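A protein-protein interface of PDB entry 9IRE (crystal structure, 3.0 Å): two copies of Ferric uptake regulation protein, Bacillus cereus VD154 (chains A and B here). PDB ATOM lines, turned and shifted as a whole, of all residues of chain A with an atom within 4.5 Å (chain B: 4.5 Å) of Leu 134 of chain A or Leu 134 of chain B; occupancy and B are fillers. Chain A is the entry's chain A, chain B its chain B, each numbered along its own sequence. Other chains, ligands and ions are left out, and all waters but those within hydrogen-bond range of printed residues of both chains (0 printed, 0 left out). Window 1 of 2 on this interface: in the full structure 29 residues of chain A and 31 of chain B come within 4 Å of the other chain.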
ATOM      1  N   HIS A  96      30.029 -17.576  -1.607  1.00  0.00           N
ATOM      2  CA  HIS A  96      29.442 -18.864  -1.974  1.00  0.00           C
ATOM      3  C   HIS A  96      30.529 -19.907  -2.322  1.00  0.00           C
ATOM      4  O   HIS A  96      31.683 -19.574  -2.635  1.00  0.00           O
ATOM      5  CB  HIS A  96      28.511 -18.684  -3.170  1.00  0.00           C
ATOM      6  CG  HIS A  96      27.579 -17.511  -3.063  1.00  0.00           C
ATOM      7  ND1 HIS A  96      27.204 -16.945  -1.859  1.00  0.00           N
ATOM      8  CD2 HIS A  96      26.943 -16.799  -4.027  1.00  0.00           C
ATOM      9  CE1 HIS A  96      26.374 -15.941  -2.095  1.00  0.00           C
ATOM     10  NE2 HIS A  96      26.203 -15.827  -3.400  1.00  0.00           N
ATOM     11  N   HIS A  97      30.167 -21.195  -2.268  1.00  0.00           N
ATOM     12  CA  HIS A  97      31.117 -22.211  -2.724  1.00  0.00           C
ATOM     13  C   HIS A  97      30.422 -23.167  -3.653  1.00  0.00           C
ATOM     14  O   HIS A  97      29.253 -23.500  -3.444  1.00  0.00           O
ATOM     15  CB  HIS A  97      31.746 -23.025  -1.593  1.00  0.00           C
ATOM     16  CG  HIS A  97      32.376 -22.171  -0.539  1.00  0.00           C
ATOM     17  ND1 HIS A  97      31.702 -21.779   0.604  1.00  0.00           N
ATOM     18  CD2 HIS A  97      33.586 -21.569  -0.478  1.00  0.00           C
ATOM     19  CE1 HIS A  97      32.487 -21.016   1.345  1.00  0.00           C
ATOM     20  NE2 HIS A  97      33.628 -20.868   0.704  1.00  0.00           N
ATOM     21  N   LEU A 114      22.733 -13.828  -4.222  1.00  0.00           N
ATOM     22  CA  LEU A 114      21.471 -14.050  -3.464  1.00  0.00           C
ATOM     23  C   LEU A 114      20.722 -12.744  -3.182  1.00  0.00           C
ATOM     24  O   LEU A 114      19.753 -12.792  -2.413  1.00  0.00           O
ATOM     25  CB  LEU A 114      21.820 -14.759  -2.159  1.00  0.00           C
ATOM     26  CG  LEU A 114      22.101 -16.257  -2.264  1.00  0.00           C
ATOM     27  CD1 LEU A 114      22.728 -16.690  -0.964  1.00  0.00           C
ATOM     28  CD2 LEU A 114      20.809 -17.010  -2.507  1.00  0.00           C
ATOM     29  N   HIS A 132      24.580 -14.753   5.020  1.00  0.00           N
ATOM     30  CA  HIS A 132      24.111 -16.036   4.501  1.00  0.00           C
ATOM     31  C   HIS A 132      25.281 -16.961   4.185  1.00  0.00           C
ATOM     32  O   HIS A 132      26.442 -16.553   4.130  1.00  0.00           O
ATOM     33  CB  HIS A 132      23.267 -15.865   3.253  1.00  0.00           C
ATOM     34  CG  HIS A 132      24.028 -15.314   2.108  1.00  0.00           C
ATOM     35  ND1 HIS A 132      23.699 -14.123   1.511  1.00  0.00           N
ATOM     36  CD2 HIS A 132      25.139 -15.757   1.482  1.00  0.00           C
ATOM     37  CE1 HIS A 132      24.560 -13.867   0.546  1.00  0.00           C
ATOM     38  NE2 HIS A 132      25.437 -14.853   0.501  1.00  0.00           N
ATOM     39  N   ARG A 133      24.939 -18.242   3.998  1.00  0.00           N
ATOM     40  CA  ARG A 133      25.949 -19.268   3.631  1.00  0.00           C
ATOM     41  C   ARG A 133      25.306 -20.135   2.540  1.00  0.00           C
ATOM     42  O   ARG A 133      24.349 -20.875   2.865  1.00  0.00           O
ATOM     43  CB  ARG A 133      26.351 -20.090   4.859  1.00  0.00           C
ATOM     44  CG  ARG A 133      27.285 -21.252   4.551  1.00  0.00           C
ATOM     45  CD  ARG A 133      28.616 -21.114   5.271  1.00  0.00           C
ATOM     46  NE  ARG A 133      28.455 -20.707   6.671  1.00  0.00           N
ATOM     47  CZ  ARG A 133      29.334 -20.970   7.628  1.00  0.00           C
ATOM     48  NH1 ARG A 133      29.253 -22.099   8.309  1.00  0.00           N
ATOM     49  NH2 ARG A 133      30.296 -20.105   7.899  1.00  0.00           N
ATOM     50  N   LEU A 134      25.787 -20.034   1.299  1.00  0.00           N
ATOM     51  CA  LEU A 134      25.186 -20.741   0.192  1.00  0.00           C
ATOM     52  C   LEU A 134      26.239 -21.702  -0.314  1.00  0.00           C
ATOM     53  O   LEU A 134      27.400 -21.307  -0.476  1.00  0.00           O
ATOM     54  CB  LEU A 134      24.741 -19.762  -0.900  1.00  0.00           C
ATOM     55  CG  LEU A 134      24.267 -20.389  -2.214  1.00  0.00           C
ATOM     56  CD1 LEU A 134      23.213 -21.398  -1.902  1.00  0.00           C
ATOM     57  CD2 LEU A 134      23.761 -19.358  -3.196  1.00  0.00           C
ATOM     58  N   THR A 135      25.862 -22.958  -0.537  1.00  0.00           N
ATOM     59  CA  THR A 135      26.820 -23.872  -1.146  1.00  0.00           C
ATOM     60  C   THR A 135      26.089 -24.757  -2.143  1.00  0.00           C
ATOM     61  O   THR A 135      24.949 -25.162  -1.900  1.00  0.00           O
ATOM     62  CB  THR A 135      27.577 -24.717  -0.091  1.00  0.00           C
ATOM     63  OG1 THR A 135      26.647 -25.334   0.785  1.00  0.00           O
ATOM     64  CG2 THR A 135      28.420 -23.842   0.761  1.00  0.00           C
ATOM     65  N   PHE A 136      26.717 -25.010  -3.286  1.00  0.00           N
ATOM     66  CA  PHE A 136      26.170 -25.950  -4.238  1.00  0.00           C
ATOM     67  C   PHE A 136      27.021 -27.197  -4.212  1.00  0.00           C
ATOM     68  O   PHE A 136      28.173 -27.181  -3.757  1.00  0.00           O
ATOM     69  CB  PHE A 136      26.141 -25.393  -5.656  1.00  0.00           C
ATOM     70  CG  PHE A 136      25.136 -24.295  -5.880  1.00  0.00           C
ATOM     71  CD1 PHE A 136      24.567 -23.615  -4.842  1.00  0.00           C
ATOM     72  CD2 PHE A 136      24.756 -23.955  -7.158  1.00  0.00           C
ATOM     73  CE1 PHE A 136      23.646 -22.607  -5.071  1.00  0.00           C
ATOM     74  CE2 PHE A 136      23.836 -22.958  -7.381  1.00  0.00           C
ATOM     75  CZ  PHE A 136      23.282 -22.283  -6.331  1.00  0.00           C
ATOM     76  N   HIS B  95      16.624 -28.336   1.671  1.00  0.00           N
ATOM     77  CA  HIS B  95      15.844 -27.137   1.957  1.00  0.00           C
ATOM     78  C   HIS B  95      16.742 -25.981   2.400  1.00  0.00           C
ATOM     79  O   HIS B  95      17.978 -26.029   2.347  1.00  0.00           O
ATOM     80  CB  HIS B  95      14.798 -27.425   3.035  1.00  0.00           C
ATOM     81  CG  HIS B  95      15.386 -27.929   4.316  1.00  0.00           C
ATOM     82  ND1 HIS B  95      15.498 -29.275   4.595  1.00  0.00           N
ATOM     83  CD2 HIS B  95      15.940 -27.280   5.369  1.00  0.00           C
ATOM     84  CE1 HIS B  95      16.075 -29.434   5.772  1.00  0.00           C
ATOM     85  NE2 HIS B  95      16.358 -28.241   6.259  1.00  0.00           N
ATOM     86  N   HIS B  96      16.088 -24.913   2.827  1.00  0.00           N
ATOM     87  CA  HIS B  96      16.748 -23.716   3.292  1.00  0.00           C
ATOM     88  C   HIS B  96      16.439 -23.530   4.781  1.00  0.00           C
ATOM     89  O   HIS B  96      15.632 -24.248   5.378  1.00  0.00           O
ATOM     90  CB  HIS B  96      16.315 -22.529   2.407  1.00  0.00           C
ATOM     91  CG  HIS B  96      16.222 -22.866   0.931  1.00  0.00           C
ATOM     92  ND1 HIS B  96      16.952 -23.885   0.342  1.00  0.00           N
ATOM     93  CD2 HIS B  96      15.469 -22.329  -0.066  1.00  0.00           C
ATOM     94  CE1 HIS B  96      16.652 -23.962  -0.945  1.00  0.00           C
ATOM     95  NE2 HIS B  96      15.753 -23.031  -1.219  1.00  0.00           N
ATOM     96  N   HIS B  97      17.147 -22.602   5.403  1.00  0.00           N
ATOM     97  CA  HIS B  97      17.050 -22.320   6.829  1.00  0.00           C
ATOM     98  C   HIS B  97      17.074 -20.817   7.039  1.00  0.00           C
ATOM     99  O   HIS B  97      17.904 -20.121   6.444  1.00  0.00           O
ATOM    100  CB  HIS B  97      18.251 -22.839   7.625  1.00  0.00           C
ATOM    101  CG  HIS B  97      18.335 -24.314   7.771  1.00  0.00           C
ATOM    102  ND1 HIS B  97      19.320 -25.049   7.149  1.00  0.00           N
ATOM    103  CD2 HIS B  97      17.672 -25.167   8.576  1.00  0.00           C
ATOM    104  CE1 HIS B  97      19.235 -26.311   7.530  1.00  0.00           C
ATOM    105  NE2 HIS B  97      18.228 -26.410   8.369  1.00  0.00           N
ATOM    106  N   LEU B 114      15.936 -20.781  -5.498  1.00  0.00           N
ATOM    107  CA  LEU B 114      17.230 -20.571  -6.138  1.00  0.00           C
ATOM    108  C   LEU B 114      17.060 -20.527  -7.640  1.00  0.00           C
ATOM    109  O   LEU B 114      17.169 -19.437  -8.217  1.00  0.00           O
ATOM    110  CB  LEU B 114      18.241 -21.640  -5.715  1.00  0.00           C
ATOM    111  CG  LEU B 114      18.716 -21.602  -4.251  1.00  0.00           C
ATOM    112  CD1 LEU B 114      20.046 -22.274  -4.087  1.00  0.00           C
ATOM    113  CD2 LEU B 114      18.800 -20.208  -3.678  1.00  0.00           C
ATOM    114  N   HIS B 132      21.821 -28.398  -2.977  1.00  0.00           N
ATOM    115  CA  HIS B 132      22.203 -27.078  -2.480  1.00  0.00           C
ATOM    116  C   HIS B 132      21.631 -26.768  -1.099  1.00  0.00           C
ATOM    117  O   HIS B 132      20.452 -27.005  -0.825  1.00  0.00           O
ATOM    118  CB  HIS B 132      21.814 -25.984  -3.481  1.00  0.00           C
ATOM    119  CG  HIS B 132      20.346 -25.732  -3.593  1.00  0.00           C
ATOM    120  ND1 HIS B 132      19.606 -26.115  -4.695  1.00  0.00           N
ATOM    121  CD2 HIS B 132      19.488 -25.088  -2.763  1.00  0.00           C
ATOM    122  CE1 HIS B 132      18.352 -25.732  -4.523  1.00  0.00           C
ATOM    123  NE2 HIS B 132      18.252 -25.120  -3.354  1.00  0.00           N
ATOM    124  N   ARG B 133      22.473 -26.176  -0.256  1.00  0.00           N
ATOM    125  CA  ARG B 133      22.151 -25.944   1.142  1.00  0.00           C
ATOM    126  C   ARG B 133      22.366 -24.474   1.495  1.00  0.00           C
ATOM    127  O   ARG B 133      23.513 -24.041   1.683  1.00  0.00           O
ATOM    128  CB  ARG B 133      22.998 -26.839   2.038  1.00  0.00           C
ATOM    129  CG  ARG B 133      22.526 -26.808   3.502  1.00  0.00           C
ATOM    130  CD  ARG B 133      23.065 -27.988   4.300  1.00  0.00           C
ATOM    131  NE  ARG B 133      24.514 -27.928   4.453  1.00  0.00           N
ATOM    132  CZ  ARG B 133      25.277 -28.941   4.838  1.00  0.00           C
ATOM    133  NH1 ARG B 133      24.767 -30.128   5.099  1.00  0.00           N
ATOM    134  NH2 ARG B 133      26.588 -28.759   4.955  1.00  0.00           N
ATOM    135  N   LEU B 134      21.271 -23.728   1.700  1.00  0.00           N
ATOM    136  CA  LEU B 134      21.363 -22.272   2.002  1.00  0.00           C
ATOM    137  C   LEU B 134      20.878 -21.971   3.424  1.00  0.00           C
ATOM    138  O   LEU B 134      19.845 -22.532   3.819  1.00  0.00           O
ATOM    139  CB  LEU B 134      20.530 -21.503   0.981  1.00  0.00           C
ATOM    140  CG  LEU B 134      20.217 -20.042   1.317  1.00  0.00           C
ATOM    141  CD1 LEU B 134      21.471 -19.198   1.216  1.00  0.00           C
ATOM    142  CD2 LEU B 134      19.145 -19.515   0.388  1.00  0.00           C
ATOM    143  N   THR B 135      21.591 -21.104   4.147  1.00  0.00           N
ATOM    144  CA  THR B 135      21.181 -20.702   5.507  1.00  0.00           C
ATOM    145  C   THR B 135      21.246 -19.200   5.613  1.00  0.00           C
ATOM    146  O   THR B 135      22.244 -18.629   5.152  1.00  0.00           O
ATOM    147  CB  THR B 135      22.090 -21.357   6.536  1.00  0.00           C
ATOM    148  OG1 THR B 135      21.772 -22.741   6.464  1.00  0.00           O
ATOM    149  CG2 THR B 135      21.832 -20.830   7.934  1.00  0.00           C
ATOM    150  N   PHE B 136      20.226 -18.578   6.204  1.00  0.00           N
ATOM    151  CA  PHE B 136      20.172 -17.100   6.333  1.00  0.00           C
ATOM    152  C   PHE B 136      20.343 -16.715   7.790  1.00  0.00           C
ATOM    153  O   PHE B 136      19.902 -17.475   8.669  1.00  0.00           O
ATOM    154  CB  PHE B 136      18.836 -16.593   5.787  1.00  0.00           C
ATOM    155  CG  PHE B 136      18.836 -16.198   4.317  1.00  0.00           C
ATOM    156  CD1 PHE B 136      19.938 -16.437   3.510  1.00  0.00           C
ATOM    157  CD2 PHE B 136      17.729 -15.588   3.743  1.00  0.00           C
ATOM    158  CE1 PHE B 136      19.934 -16.072   2.175  1.00  0.00           C
ATOM    159  CE2 PHE B 136      17.733 -15.226   2.405  1.00  0.00           C
ATOM    160  CZ  PHE B 136      18.832 -15.470   1.624  1.00  0.00           C
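The backbone NH of Arg 133 of chain A lies within hydrogen-bond range of the backbone carbonyl oxygen of Thr 135 of chain B, at 3.0 Å. The backbone carbonyl oxygen of Arg 133 of chain A sits close to the backbone carbonyl oxygen of Arg 133 of chain B (3.5 Å). N of Arg 133 of chain B lies within hydrogen-bond range of O of Thr 135 of chain A (3.1 Å).
O of His 97 of chain A lies within hydrogen-bond range of N of Phe 136 of chain A. The backbone carbonyl oxygen of His 97 of chain B lies within hydrogen-bond range of the backbone NH of Phe 136 of chain B. O of Leu 134 of chain B sits at hydrogen-bond distance from N of His 97 of chain B. The backbone carbonyl oxygen (O) of Leu 134 of chain A sits at hydrogen-bond distance from the backbone NH (N) of His 97 of chain A, 3.3 Å away. ND1 of His 97 of chain B is in hydrogen-bond range of OG1 of Thr 135 of chain B (3.4 Å).
Among the printed residues, pairs that only touch across the chains: Leu 114 of chain A with Leu 114 of chain B, Leu 114 of chain A with Leu 134 of chain B, His 132 of chain A with Thr 135 of chain B, His 132 of chain A with Phe 136 of chain B, Arg 133 of chain A with Leu 134 of chain B, Leu 134 of chain A with Leu 114 of chain B, Leu 134 of chain A with Arg 133 of chain B, Leu 134 of chain A with Leu 134 of chain B, Thr 135 of chain A with His 132 of chain B, Phe 136 of chain A with Leu 114 of chain B and Phe 136 of chain A with His 132 of chain B.
Printed residues of chain B within 4 Å of Arg 133 of chain A: Arg 133 (3.5 Å), Leu 134 (3.4 Å) and Thr 135 (3.0 Å). Of the printed residues of chain B, Leu 134 of chain A touches Leu 114, Arg 133 and Leu 134. Of the printed residues of chain A, Leu 114 of chain B touches Leu 114 (3.95 Å), Leu 134 (3.9 Å) and Phe 136 (3.7 Å). Printed residues of chain A within 4 Å of Arg 133 of chain B: Arg 133 (3.5 Å), Leu 134 (3.99 Å) and Thr 135 (3.1 Å). Printed residues of chain A within 4 Å of Leu 134 of chain B: Leu 114, Arg 133 and Leu 134. Of the printed residues of chain A, Thr 135 of chain B touches His 132 (3.3 Å) and Arg 133 (3.0 Å). Printed residues of chain A within 4 Å of Phe 136 of chain B: His 132 (3.4 Å). The nearest residue of chain A that does not touch Leu 134 of chain B is His 132 of chain A (4.3 Å). The nearest printed residue of chain A that does not touch Arg 133 of chain B is Phe 136 of chain A (5.3 Å).
Of the 8 printed residues of chain A, 6 touch a printed residue of chain B. Hydrophobic or aromatic side chains of chain B that line the printed part of chain A: Leu 114, His 132, Leu 134 and Phe 136. Among the printed residues, no Asp or Glu carboxylate lies within 4 Å of a Lys or Arg side-chain nitrogen of the other chain.
Leu 114 of chain B touches its own counterpart, Leu 114 of chain A. Leu 114 of chain A touches Leu 134 of chain B, and with the chains exchanged Leu 134 of chain A touches Leu 114 of chain B. Arg 133 of chain A touches Leu 134 of chain B, and with the chains exchanged Leu 134 of chain A touches Arg 133 of chain B. Arg 133 of chain A touches Thr 135 of chain B, and with the chains exchanged Thr 135 of chain A touches Arg 133 of chain B. 8 positions are printed for both chains.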
